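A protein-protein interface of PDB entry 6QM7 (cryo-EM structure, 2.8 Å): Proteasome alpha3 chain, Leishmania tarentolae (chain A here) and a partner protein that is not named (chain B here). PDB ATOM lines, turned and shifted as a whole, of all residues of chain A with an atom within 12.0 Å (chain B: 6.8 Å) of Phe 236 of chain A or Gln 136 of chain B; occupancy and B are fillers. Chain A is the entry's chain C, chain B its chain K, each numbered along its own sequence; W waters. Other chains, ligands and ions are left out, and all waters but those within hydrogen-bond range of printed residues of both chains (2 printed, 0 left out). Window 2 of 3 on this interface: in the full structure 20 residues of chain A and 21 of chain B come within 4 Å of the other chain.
N of Tyr 128 of chain B sits at hydrogen-bond distance from O of Gln 136 of chain B (2.8 Å).
The side-chain amide nitrogen (NE2) of Gln 231 of chain A is in hydrogen-bond range of the backbone carbonyl oxygen (O) of Lys 237 of chain A.
Of the printed residues of chain B, Lys 237 of chain A touches Glu 80 (3.7 Å).
Printed residues of chain B within 4 Å of His 238 of chain A: Val 121.
Arg 9 of chain B touches none of the printed residues of chain A.
Of the printed residues of chain A, Glu 80 of chain B touches Lys 237.
Of the printed residues of chain A, Val 121 of chain B touches His 238.
No residue of chain A comes within 4 Å of Phe 127 of chain B.
No residue of chain A comes within 4 Å of Met 129 of chain B.
No residue of chain A comes within 4 Å of Thr 134 of chain B.
No residue of chain A comes within 4 Å of Leu 135 of chain B.
Of chain A, only Phe 236 comes within 4 Å of Gln 136 of chain B.
No residue of chain A comes within 4 Å of Val 138 of chain B.
Pro 139 of chain B touches none of the printed residues of chain A.
The nearest residue of chain B that does not touch Phe 236 of chain A is Arg 9 of chain B (4.4 Å).
Among the printed residues, merely in contact across the chains: His 238 of chain A with Val 121 of chain B (3.5 Å), Phe 236 of chain A with Ala 137 of chain B (3.5 Å), Lys 237 of chain A with Glu 80 of chain B (3.7 Å) and Phe 236 of chain A with Gln 136 of chain B (3.9 Å).
Water W1 lies within hydrogen-bond range of the backbone carbonyl oxygen of Phe 236 of chain A (2.9 Å) and the side-chain amide nitrogen of Gln 125 of chain B (3.2 Å).
Water W2 lies within hydrogen-bond range of the side-chain carboxylate of Asp 234 of chain A and the side-chain amide nitrogen of Gln 136 of chain B.
Of the 16 printed residues of chain B, 4 touch a printed residue of chain A.
Printed residues of chain B that touch a printed residue of chain A: Glu 80, Val 121, Gln 136 and Ala 137.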
ATOM      1  N   GLN A 108     -28.172 -32.391 -21.984  1.00  0.00           N
ATOM      2  CA  GLN A 108     -27.785 -31.558 -23.161  1.00  0.00           C
ATOM      3  C   GLN A 108     -27.162 -32.457 -24.226  1.00  0.00           C
ATOM      4  O   GLN A 108     -26.188 -32.038 -24.863  1.00  0.00           O
ATOM      5  CB  GLN A 108     -26.871 -30.399 -22.751  1.00  0.00           C
ATOM      6  CG  GLN A 108     -27.564 -29.368 -21.861  1.00  0.00           C
ATOM      7  CD  GLN A 108     -28.809 -28.782 -22.491  1.00  0.00           C
ATOM      8  OE1 GLN A 108     -28.809 -28.385 -23.659  1.00  0.00           O
ATOM      9  NE2 GLN A 108     -29.890 -28.731 -21.728  1.00  0.00           N
ATOM     10  N   ILE A 229     -24.468 -24.824 -38.018  1.00  0.00           N
ATOM     11  CA  ILE A 229     -23.438 -25.137 -36.983  1.00  0.00           C
ATOM     12  C   ILE A 229     -23.542 -24.051 -35.897  1.00  0.00           C
ATOM     13  O   ILE A 229     -23.847 -24.408 -34.739  1.00  0.00           O
ATOM     14  CB  ILE A 229     -22.014 -25.236 -37.592  1.00  0.00           C
ATOM     15  CG1 ILE A 229     -21.931 -26.133 -38.836  1.00  0.00           C
ATOM     16  CG2 ILE A 229     -21.001 -25.675 -36.544  1.00  0.00           C
ATOM     17  CD1 ILE A 229     -22.109 -27.613 -38.567  1.00  0.00           C
ATOM     18  N   ASP A 230     -23.340 -22.779 -36.284  1.00  0.00           N
ATOM     19  CA  ASP A 230     -23.280 -21.570 -35.407  1.00  0.00           C
ATOM     20  C   ASP A 230     -22.129 -21.746 -34.405  1.00  0.00           C
ATOM     21  O   ASP A 230     -22.362 -21.566 -33.192  1.00  0.00           O
ATOM     22  CB  ASP A 230     -24.629 -21.274 -34.729  1.00  0.00           C
ATOM     23  CG  ASP A 230     -25.737 -20.783 -35.657  1.00  0.00           C
ATOM     24  OD1 ASP A 230     -25.427 -20.039 -36.613  1.00  0.00           O
ATOM     25  OD2 ASP A 230     -26.909 -21.136 -35.409  1.00  0.00           O
ATOM     26  N   GLN A 231     -20.931 -22.069 -34.910  1.00  0.00           N
ATOM     27  CA  GLN A 231     -19.738 -22.460 -34.105  1.00  0.00           C
ATOM     28  C   GLN A 231     -19.264 -21.281 -33.241  1.00  0.00           C
ATOM     29  O   GLN A 231     -18.768 -21.549 -32.133  1.00  0.00           O
ATOM     30  CB  GLN A 231     -18.601 -22.959 -35.008  1.00  0.00           C
ATOM     31  CG  GLN A 231     -17.384 -23.525 -34.270  1.00  0.00           C
ATOM     32  CD  GLN A 231     -17.657 -24.818 -33.539  1.00  0.00           C
ATOM     33  OE1 GLN A 231     -17.832 -25.870 -34.149  1.00  0.00           O
ATOM     34  NE2 GLN A 231     -17.688 -24.752 -32.218  1.00  0.00           N
ATOM     35  N   LEU A 232     -19.401 -20.038 -33.709  1.00  0.00           N
ATOM     36  CA  LEU A 232     -18.896 -18.842 -32.986  1.00  0.00           C
ATOM     37  C   LEU A 232     -19.738 -18.551 -31.740  1.00  0.00           C
ATOM     38  O   LEU A 232     -19.240 -17.783 -30.892  1.00  0.00           O
ATOM     39  CB  LEU A 232     -18.914 -17.626 -33.911  1.00  0.00           C
ATOM     40  CG  LEU A 232     -18.015 -17.707 -35.140  1.00  0.00           C
ATOM     41  CD1 LEU A 232     -18.069 -16.404 -35.916  1.00  0.00           C
ATOM     42  CD2 LEU A 232     -16.584 -18.034 -34.750  1.00  0.00           C
ATOM     43  N   LEU A 233     -20.951 -19.103 -31.626  1.00  0.00           N
ATOM     44  CA  LEU A 233     -21.855 -18.855 -30.469  1.00  0.00           C
ATOM     45  C   LEU A 233     -21.485 -19.741 -29.271  1.00  0.00           C
ATOM     46  O   LEU A 233     -21.729 -19.299 -28.122  1.00  0.00           O
ATOM     47  CB  LEU A 233     -23.306 -19.094 -30.880  1.00  0.00           C
ATOM     48  CG  LEU A 233     -23.899 -18.097 -31.869  1.00  0.00           C
ATOM     49  CD1 LEU A 233     -25.410 -18.232 -31.887  1.00  0.00           C
ATOM     50  CD2 LEU A 233     -23.511 -16.667 -31.542  1.00  0.00           C
ATOM     51  N   ASP A 234     -20.960 -20.942 -29.522  1.00  0.00           N
ATOM     52  CA  ASP A 234     -20.331 -21.805 -28.487  1.00  0.00           C
ATOM     53  C   ASP A 234     -19.048 -22.391 -29.079  1.00  0.00           C
ATOM     54  O   ASP A 234     -19.076 -23.440 -29.722  1.00  0.00           O
ATOM     55  CB  ASP A 234     -21.337 -22.826 -27.947  1.00  0.00           C
ATOM     56  CG  ASP A 234     -21.087 -23.229 -26.498  1.00  0.00           C
ATOM     57  OD1 ASP A 234     -19.896 -23.298 -26.089  1.00  0.00           O
ATOM     58  OD2 ASP A 234     -22.085 -23.466 -25.780  1.00  0.00           O
ATOM     59  N   PRO A 235     -17.896 -21.694 -28.927  1.00  0.00           N
ATOM     60  CA  PRO A 235     -16.621 -22.147 -29.490  1.00  0.00           C
ATOM     61  C   PRO A 235     -16.160 -23.559 -29.107  1.00  0.00           C
ATOM     62  O   PRO A 235     -15.477 -24.177 -29.895  1.00  0.00           O
ATOM     63  CB  PRO A 235     -15.594 -21.155 -28.919  1.00  0.00           C
ATOM     64  CG  PRO A 235     -16.396 -19.901 -28.650  1.00  0.00           C
ATOM     65  CD  PRO A 235     -17.772 -20.391 -28.258  1.00  0.00           C
ATOM     66  N   PHE A 236     -16.527 -24.016 -27.912  1.00  0.00           N
ATOM     67  CA  PHE A 236     -16.063 -25.293 -27.321  1.00  0.00           C
ATOM     68  C   PHE A 236     -17.032 -26.434 -27.644  1.00  0.00           C
ATOM     69  O   PHE A 236     -16.662 -27.595 -27.405  1.00  0.00           O
ATOM     70  CB  PHE A 236     -15.861 -25.101 -25.820  1.00  0.00           C
ATOM     71  CG  PHE A 236     -14.758 -24.127 -25.495  1.00  0.00           C
ATOM     72  CD1 PHE A 236     -13.436 -24.548 -25.442  1.00  0.00           C
ATOM     73  CD2 PHE A 236     -15.035 -22.786 -25.269  1.00  0.00           C
ATOM     74  CE1 PHE A 236     -12.419 -23.649 -25.150  1.00  0.00           C
ATOM     75  CE2 PHE A 236     -14.016 -21.889 -24.980  1.00  0.00           C
ATOM     76  CZ  PHE A 236     -12.710 -22.320 -24.924  1.00  0.00           C
ATOM     77  N   LYS A 237     -18.216 -26.132 -28.172  1.00  0.00           N
ATOM     78  CA  LYS A 237     -19.233 -27.161 -28.506  1.00  0.00           C
ATOM     79  C   LYS A 237     -18.797 -27.859 -29.797  1.00  0.00           C
ATOM     80  O   LYS A 237     -18.498 -27.152 -30.785  1.00  0.00           O
ATOM     81  CB  LYS A 237     -20.633 -26.539 -28.602  1.00  0.00           C
ATOM     82  CG  LYS A 237     -21.775 -27.397 -28.062  1.00  0.00           C
ATOM     83  CD  LYS A 237     -22.618 -28.069 -29.134  1.00  0.00           C
ATOM     84  CE  LYS A 237     -23.372 -29.291 -28.642  1.00  0.00           C
ATOM     85  NZ  LYS A 237     -24.425 -28.937 -27.659  1.00  0.00           N
ATOM     86  N   HIS A 238     -18.710 -29.191 -29.763  1.00  0.00           N
ATOM     87  CA  HIS A 238     -18.448 -30.052 -30.945  1.00  0.00           C
ATOM     88  C   HIS A 238     -19.771 -30.323 -31.653  1.00  0.00           C
ATOM     89  O   HIS A 238     -20.662 -30.908 -31.023  1.00  0.00           O
ATOM     90  CB  HIS A 238     -17.776 -31.372 -30.559  1.00  0.00           C
ATOM     91  CG  HIS A 238     -17.537 -32.277 -31.725  1.00  0.00           C
ATOM     92  ND1 HIS A 238     -16.490 -32.076 -32.620  1.00  0.00           N
ATOM     93  CD2 HIS A 238     -18.193 -33.381 -32.147  1.00  0.00           C
ATOM     94  CE1 HIS A 238     -16.514 -33.018 -33.539  1.00  0.00           C
ATOM     95  NE2 HIS A 238     -17.549 -33.835 -33.268  1.00  0.00           N
ATOM     96  N   HIS A 239     -19.878 -29.896 -32.908  1.00  0.00           N
ATOM     97  CA  HIS A 239     -21.020 -30.180 -33.807  1.00  0.00           C
ATOM     98  C   HIS A 239     -20.591 -31.303 -34.740  1.00  0.00           C
ATOM     99  O   HIS A 239     -19.607 -31.149 -35.458  1.00  0.00           O
ATOM    100  CB  HIS A 239     -21.456 -28.902 -34.531  1.00  0.00           C
ATOM    101  CG  HIS A 239     -21.840 -27.799 -33.601  1.00  0.00           C
ATOM    102  ND1 HIS A 239     -23.042 -27.797 -32.916  1.00  0.00           N
ATOM    103  CD2 HIS A 239     -21.186 -26.671 -33.233  1.00  0.00           C
ATOM    104  CE1 HIS A 239     -23.117 -26.712 -32.170  1.00  0.00           C
ATOM    105  NE2 HIS A 239     -21.985 -26.005 -32.344  1.00  0.00           N
ATOM    106  N   PRO A 240     -21.266 -32.474 -34.718  1.00  0.00           N
ATOM    107  CA  PRO A 240     -20.998 -33.535 -35.689  1.00  0.00           C
ATOM    108  C   PRO A 240     -21.265 -33.094 -37.136  1.00  0.00           C
ATOM    109  O   PRO A 240     -22.128 -32.254 -37.351  1.00  0.00           O
ATOM    110  CB  PRO A 240     -21.965 -34.654 -35.288  1.00  0.00           C
ATOM    111  CG  PRO A 240     -22.274 -34.375 -33.833  1.00  0.00           C
ATOM    112  CD  PRO A 240     -22.286 -32.866 -33.735  1.00  0.00           C
ATOM    113  N   ARG B   9      -5.892 -28.976 -19.642  1.00  0.00           N
ATOM    114  CA  ARG B   9      -6.279 -29.921 -20.700  1.00  0.00           C
ATOM    115  C   ARG B   9      -5.306 -29.718 -21.831  1.00  0.00           C
ATOM    116  O   ARG B   9      -5.148 -28.581 -22.224  1.00  0.00           O
ATOM    117  CB  ARG B   9      -7.684 -29.564 -21.157  1.00  0.00           C
ATOM    118  CG  ARG B   9      -8.269 -30.512 -22.185  1.00  0.00           C
ATOM    119  CD  ARG B   9      -9.330 -29.775 -22.974  1.00  0.00           C
ATOM    120  NE  ARG B   9      -8.697 -28.733 -23.768  1.00  0.00           N
ATOM    121  CZ  ARG B   9      -9.265 -27.588 -24.122  1.00  0.00           C
ATOM    122  NH1 ARG B   9     -10.504 -27.293 -23.743  1.00  0.00           N
ATOM    123  NH2 ARG B   9      -8.572 -26.723 -24.846  1.00  0.00           N
ATOM    124  N   GLU B  80     -19.632 -34.013 -21.667  1.00  0.00           N
ATOM    125  CA  GLU B  80     -20.662 -32.943 -21.796  1.00  0.00           C
ATOM    126  C   GLU B  80     -21.894 -33.375 -21.000  1.00  0.00           C
ATOM    127  O   GLU B  80     -22.384 -32.568 -20.186  1.00  0.00           O
ATOM    128  CB  GLU B  80     -21.059 -32.665 -23.251  1.00  0.00           C
ATOM    129  CG  GLU B  80     -20.169 -31.640 -23.960  1.00  0.00           C
ATOM    130  CD  GLU B  80     -20.776 -30.263 -24.226  1.00  0.00           C
ATOM    131  OE1 GLU B  80     -20.891 -29.880 -25.423  1.00  0.00           O
ATOM    132  OE2 GLU B  80     -21.127 -29.562 -23.246  1.00  0.00           O
ATOM    133  N   VAL B 121     -17.273 -35.904 -29.926  1.00  0.00           N
ATOM    134  CA  VAL B 121     -15.937 -35.424 -29.453  1.00  0.00           C
ATOM    135  C   VAL B 121     -15.099 -36.642 -29.087  1.00  0.00           C
ATOM    136  O   VAL B 121     -15.576 -37.467 -28.289  1.00  0.00           O
ATOM    137  CB  VAL B 121     -15.947 -34.454 -28.248  1.00  0.00           C
ATOM    138  CG1 VAL B 121     -15.156 -33.190 -28.562  1.00  0.00           C
ATOM    139  CG2 VAL B 121     -17.327 -34.114 -27.696  1.00  0.00           C
ATOM    140  N   GLN B 125     -11.591 -33.408 -22.133  1.00  0.00           N
ATOM    141  CA  GLN B 125     -12.620 -32.383 -21.878  1.00  0.00           C
ATOM    142  C   GLN B 125     -12.397 -31.870 -20.455  1.00  0.00           C
ATOM    143  O   GLN B 125     -12.037 -32.662 -19.582  1.00  0.00           O
ATOM    144  CB  GLN B 125     -13.998 -33.020 -22.018  1.00  0.00           C
ATOM    145  CG  GLN B 125     -14.295 -33.586 -23.400  1.00  0.00           C
ATOM    146  CD  GLN B 125     -14.850 -32.522 -24.314  1.00  0.00           C
ATOM    147  OE1 GLN B 125     -15.908 -31.938 -24.059  1.00  0.00           O
ATOM    148  NE2 GLN B 125     -14.122 -32.256 -25.386  1.00  0.00           N
ATOM    149  N   LEU B 126     -12.559 -30.579 -20.250  1.00  0.00           N
ATOM    150  CA  LEU B 126     -12.426 -29.953 -18.924  1.00  0.00           C
ATOM    151  C   LEU B 126     -13.533 -28.923 -18.793  1.00  0.00           C
ATOM    152  O   LEU B 126     -13.728 -28.161 -19.738  1.00  0.00           O
ATOM    153  CB  LEU B 126     -11.049 -29.311 -18.809  1.00  0.00           C
ATOM    154  CG  LEU B 126     -10.790 -28.583 -17.497  1.00  0.00           C
ATOM    155  CD1 LEU B 126     -10.851 -29.528 -16.308  1.00  0.00           C
ATOM    156  CD2 LEU B 126      -9.444 -27.913 -17.535  1.00  0.00           C
ATOM    157  N   PHE B 127     -14.234 -28.943 -17.670  1.00  0.00           N
ATOM    158  CA  PHE B 127     -15.399 -28.085 -17.392  1.00  0.00           C
ATOM    159  C   PHE B 127     -15.227 -27.451 -16.025  1.00  0.00           C
ATOM    160  O   PHE B 127     -15.196 -28.165 -15.021  1.00  0.00           O
ATOM    161  CB  PHE B 127     -16.664 -28.926 -17.423  1.00  0.00           C
ATOM    162  CG  PHE B 127     -17.020 -29.381 -18.806  1.00  0.00           C
ATOM    163  CD1 PHE B 127     -17.753 -28.561 -19.641  1.00  0.00           C
ATOM    164  CD2 PHE B 127     -16.590 -30.614 -19.273  1.00  0.00           C
ATOM    165  CE1 PHE B 127     -18.065 -28.975 -20.920  1.00  0.00           C
ATOM    166  CE2 PHE B 127     -16.915 -31.037 -20.550  1.00  0.00           C
ATOM    167  CZ  PHE B 127     -17.650 -30.212 -21.369  1.00  0.00           C
ATOM    168  N   TYR B 128     -15.102 -26.137 -16.005  1.00  0.00           N
ATOM    169  CA  TYR B 128     -15.145 -25.328 -14.766  1.00  0.00           C
ATOM    170  C   TYR B 128     -16.596 -25.307 -14.302  1.00  0.00           C
ATOM    171  O   TYR B 128     -17.445 -25.168 -15.176  1.00  0.00           O
ATOM    172  CB  TYR B 128     -14.533 -23.970 -15.081  1.00  0.00           C
ATOM    173  CG  TYR B 128     -14.669 -22.948 -13.993  1.00  0.00           C
ATOM    174  CD1 TYR B 128     -13.590 -22.607 -13.189  1.00  0.00           C
ATOM    175  CD2 TYR B 128     -15.870 -22.285 -13.804  1.00  0.00           C
ATOM    176  CE1 TYR B 128     -13.709 -21.645 -12.200  1.00  0.00           C
ATOM    177  CE2 TYR B 128     -16.013 -21.344 -12.802  1.00  0.00           C
ATOM    178  CZ  TYR B 128     -14.928 -21.012 -12.008  1.00  0.00           C
ATOM    179  OH  TYR B 128     -15.082 -20.068 -11.033  1.00  0.00           O
ATOM    180  N   MET B 129     -16.876 -25.513 -13.015  1.00  0.00           N
ATOM    181  CA  MET B 129     -18.255 -25.390 -12.468  1.00  0.00           C
ATOM    182  C   MET B 129     -18.212 -24.662 -11.137  1.00  0.00           C
ATOM    183  O   MET B 129     -17.510 -25.116 -10.250  1.00  0.00           O
ATOM    184  CB  MET B 129     -18.979 -26.726 -12.283  1.00  0.00           C
ATOM    185  CG  MET B 129     -18.479 -27.826 -13.214  1.00  0.00           C
ATOM    186  SD  MET B 129     -19.585 -29.234 -13.582  1.00  0.00           S
ATOM    187  CE  MET B 129     -20.993 -28.826 -12.550  1.00  0.00           C
ATOM    188  N   ASP B 130     -18.939 -23.559 -11.033  1.00  0.00           N
ATOM    189  CA  ASP B 130     -19.170 -22.823  -9.767  1.00  0.00           C
ATOM    190  C   ASP B 130     -20.178 -23.645  -8.975  1.00  0.00           C
ATOM    191  O   ASP B 130     -20.806 -24.524  -9.559  1.00  0.00           O
ATOM    192  CB  ASP B 130     -19.670 -21.397 -10.048  1.00  0.00           C
ATOM    193  CG  ASP B 130     -19.301 -20.321  -9.026  1.00  0.00           C
ATOM    194  OD1 ASP B 130     -20.020 -19.285  -8.987  1.00  0.00           O
ATOM    195  OD2 ASP B 130     -18.284 -20.488  -8.299  1.00  0.00           O
ATOM    196  N   GLY B 133     -23.823 -23.505 -10.218  1.00  0.00           N
ATOM    197  CA  GLY B 133     -24.200 -24.335 -11.373  1.00  0.00           C
ATOM    198  C   GLY B 133     -23.709 -23.762 -12.686  1.00  0.00           C
ATOM    199  O   GLY B 133     -24.108 -24.280 -13.738  1.00  0.00           O
ATOM    200  N   THR B 134     -22.908 -22.703 -12.631  1.00  0.00           N
ATOM    201  CA  THR B 134     -22.169 -22.144 -13.780  1.00  0.00           C
ATOM    202  C   THR B 134     -21.311 -23.254 -14.383  1.00  0.00           C
ATOM    203  O   THR B 134     -20.386 -23.664 -13.706  1.00  0.00           O
ATOM    204  CB  THR B 134     -21.251 -21.014 -13.307  1.00  0.00           C
ATOM    205  OG1 THR B 134     -22.046 -20.031 -12.633  1.00  0.00           O
ATOM    206  CG2 THR B 134     -20.449 -20.420 -14.445  1.00  0.00           C
ATOM    207  N   LEU B 135     -21.620 -23.733 -15.579  1.00  0.00           N
ATOM    208  CA  LEU B 135     -20.754 -24.671 -16.336  1.00  0.00           C
ATOM    209  C   LEU B 135     -20.045 -23.901 -17.446  1.00  0.00           C
ATOM    210  O   LEU B 135     -20.715 -23.129 -18.149  1.00  0.00           O
ATOM    211  CB  LEU B 135     -21.650 -25.767 -16.920  1.00  0.00           C
ATOM    212  CG  LEU B 135     -20.947 -26.882 -17.683  1.00  0.00           C
ATOM    213  CD1 LEU B 135     -20.011 -27.630 -16.756  1.00  0.00           C
ATOM    214  CD2 LEU B 135     -21.961 -27.843 -18.292  1.00  0.00           C
ATOM    215  N   GLN B 136     -18.746 -24.098 -17.613  1.00  0.00           N
ATOM    216  CA  GLN B 136     -17.987 -23.512 -18.748  1.00  0.00           C
ATOM    217  C   GLN B 136     -16.886 -24.469 -19.166  1.00  0.00           C
ATOM    218  O   GLN B 136     -16.089 -24.848 -18.311  1.00  0.00           O
ATOM    219  CB  GLN B 136     -17.360 -22.167 -18.375  1.00  0.00           C
ATOM    220  CG  GLN B 136     -16.736 -21.385 -19.537  1.00  0.00           C
ATOM    221  CD  GLN B 136     -17.480 -21.458 -20.851  1.00  0.00           C
ATOM    222  OE1 GLN B 136     -18.695 -21.264 -20.913  1.00  0.00           O
ATOM    223  NE2 GLN B 136     -16.757 -21.741 -21.923  1.00  0.00           N
ATOM    224  N   ALA B 137     -16.848 -24.839 -20.435  1.00  0.00           N
ATOM    225  CA  ALA B 137     -15.679 -25.542 -20.986  1.00  0.00           C
ATOM    226  C   ALA B 137     -14.500 -24.577 -20.889  1.00  0.00           C
ATOM    227  O   ALA B 137     -14.681 -23.380 -21.186  1.00  0.00           O
ATOM    228  CB  ALA B 137     -15.923 -25.998 -22.399  1.00  0.00           C
ATOM    229  N   VAL B 138     -13.351 -25.075 -20.451  1.00  0.00           N
ATOM    230  CA  VAL B 138     -12.109 -24.268 -20.352  1.00  0.00           C
ATOM    231  C   VAL B 138     -10.931 -25.150 -20.725  1.00  0.00           C
ATOM    232  O   VAL B 138     -10.993 -26.361 -20.562  1.00  0.00           O
ATOM    233  CB  VAL B 138     -11.924 -23.684 -18.945  1.00  0.00           C
ATOM    234  CG1 VAL B 138     -13.058 -22.736 -18.565  1.00  0.00           C
ATOM    235  CG2 VAL B 138     -11.732 -24.767 -17.891  1.00  0.00           C
ATOM    236  N   PRO B 139      -9.826 -24.561 -21.223  1.00  0.00           N
ATOM    237  CA  PRO B 139      -8.585 -25.300 -21.427  1.00  0.00           C
ATOM    238  C   PRO B 139      -7.880 -25.571 -20.097  1.00  0.00           C
ATOM    239  O   PRO B 139      -7.125 -26.486 -20.011  1.00  0.00           O
ATOM    240  CB  PRO B 139      -7.778 -24.351 -22.307  1.00  0.00           C
ATOM    241  CG  PRO B 139      -8.221 -23.006 -21.823  1.00  0.00           C
ATOM    242  CD  PRO B 139      -9.707 -23.150 -21.593  1.00  0.00           C
HETATM  243  O   HOH W   1     -15.374 -30.171 -27.535  1.00  0.00           O
HETATM  244  O   HOH W   2     -18.066 -21.248 -24.899  1.00  0.00           O
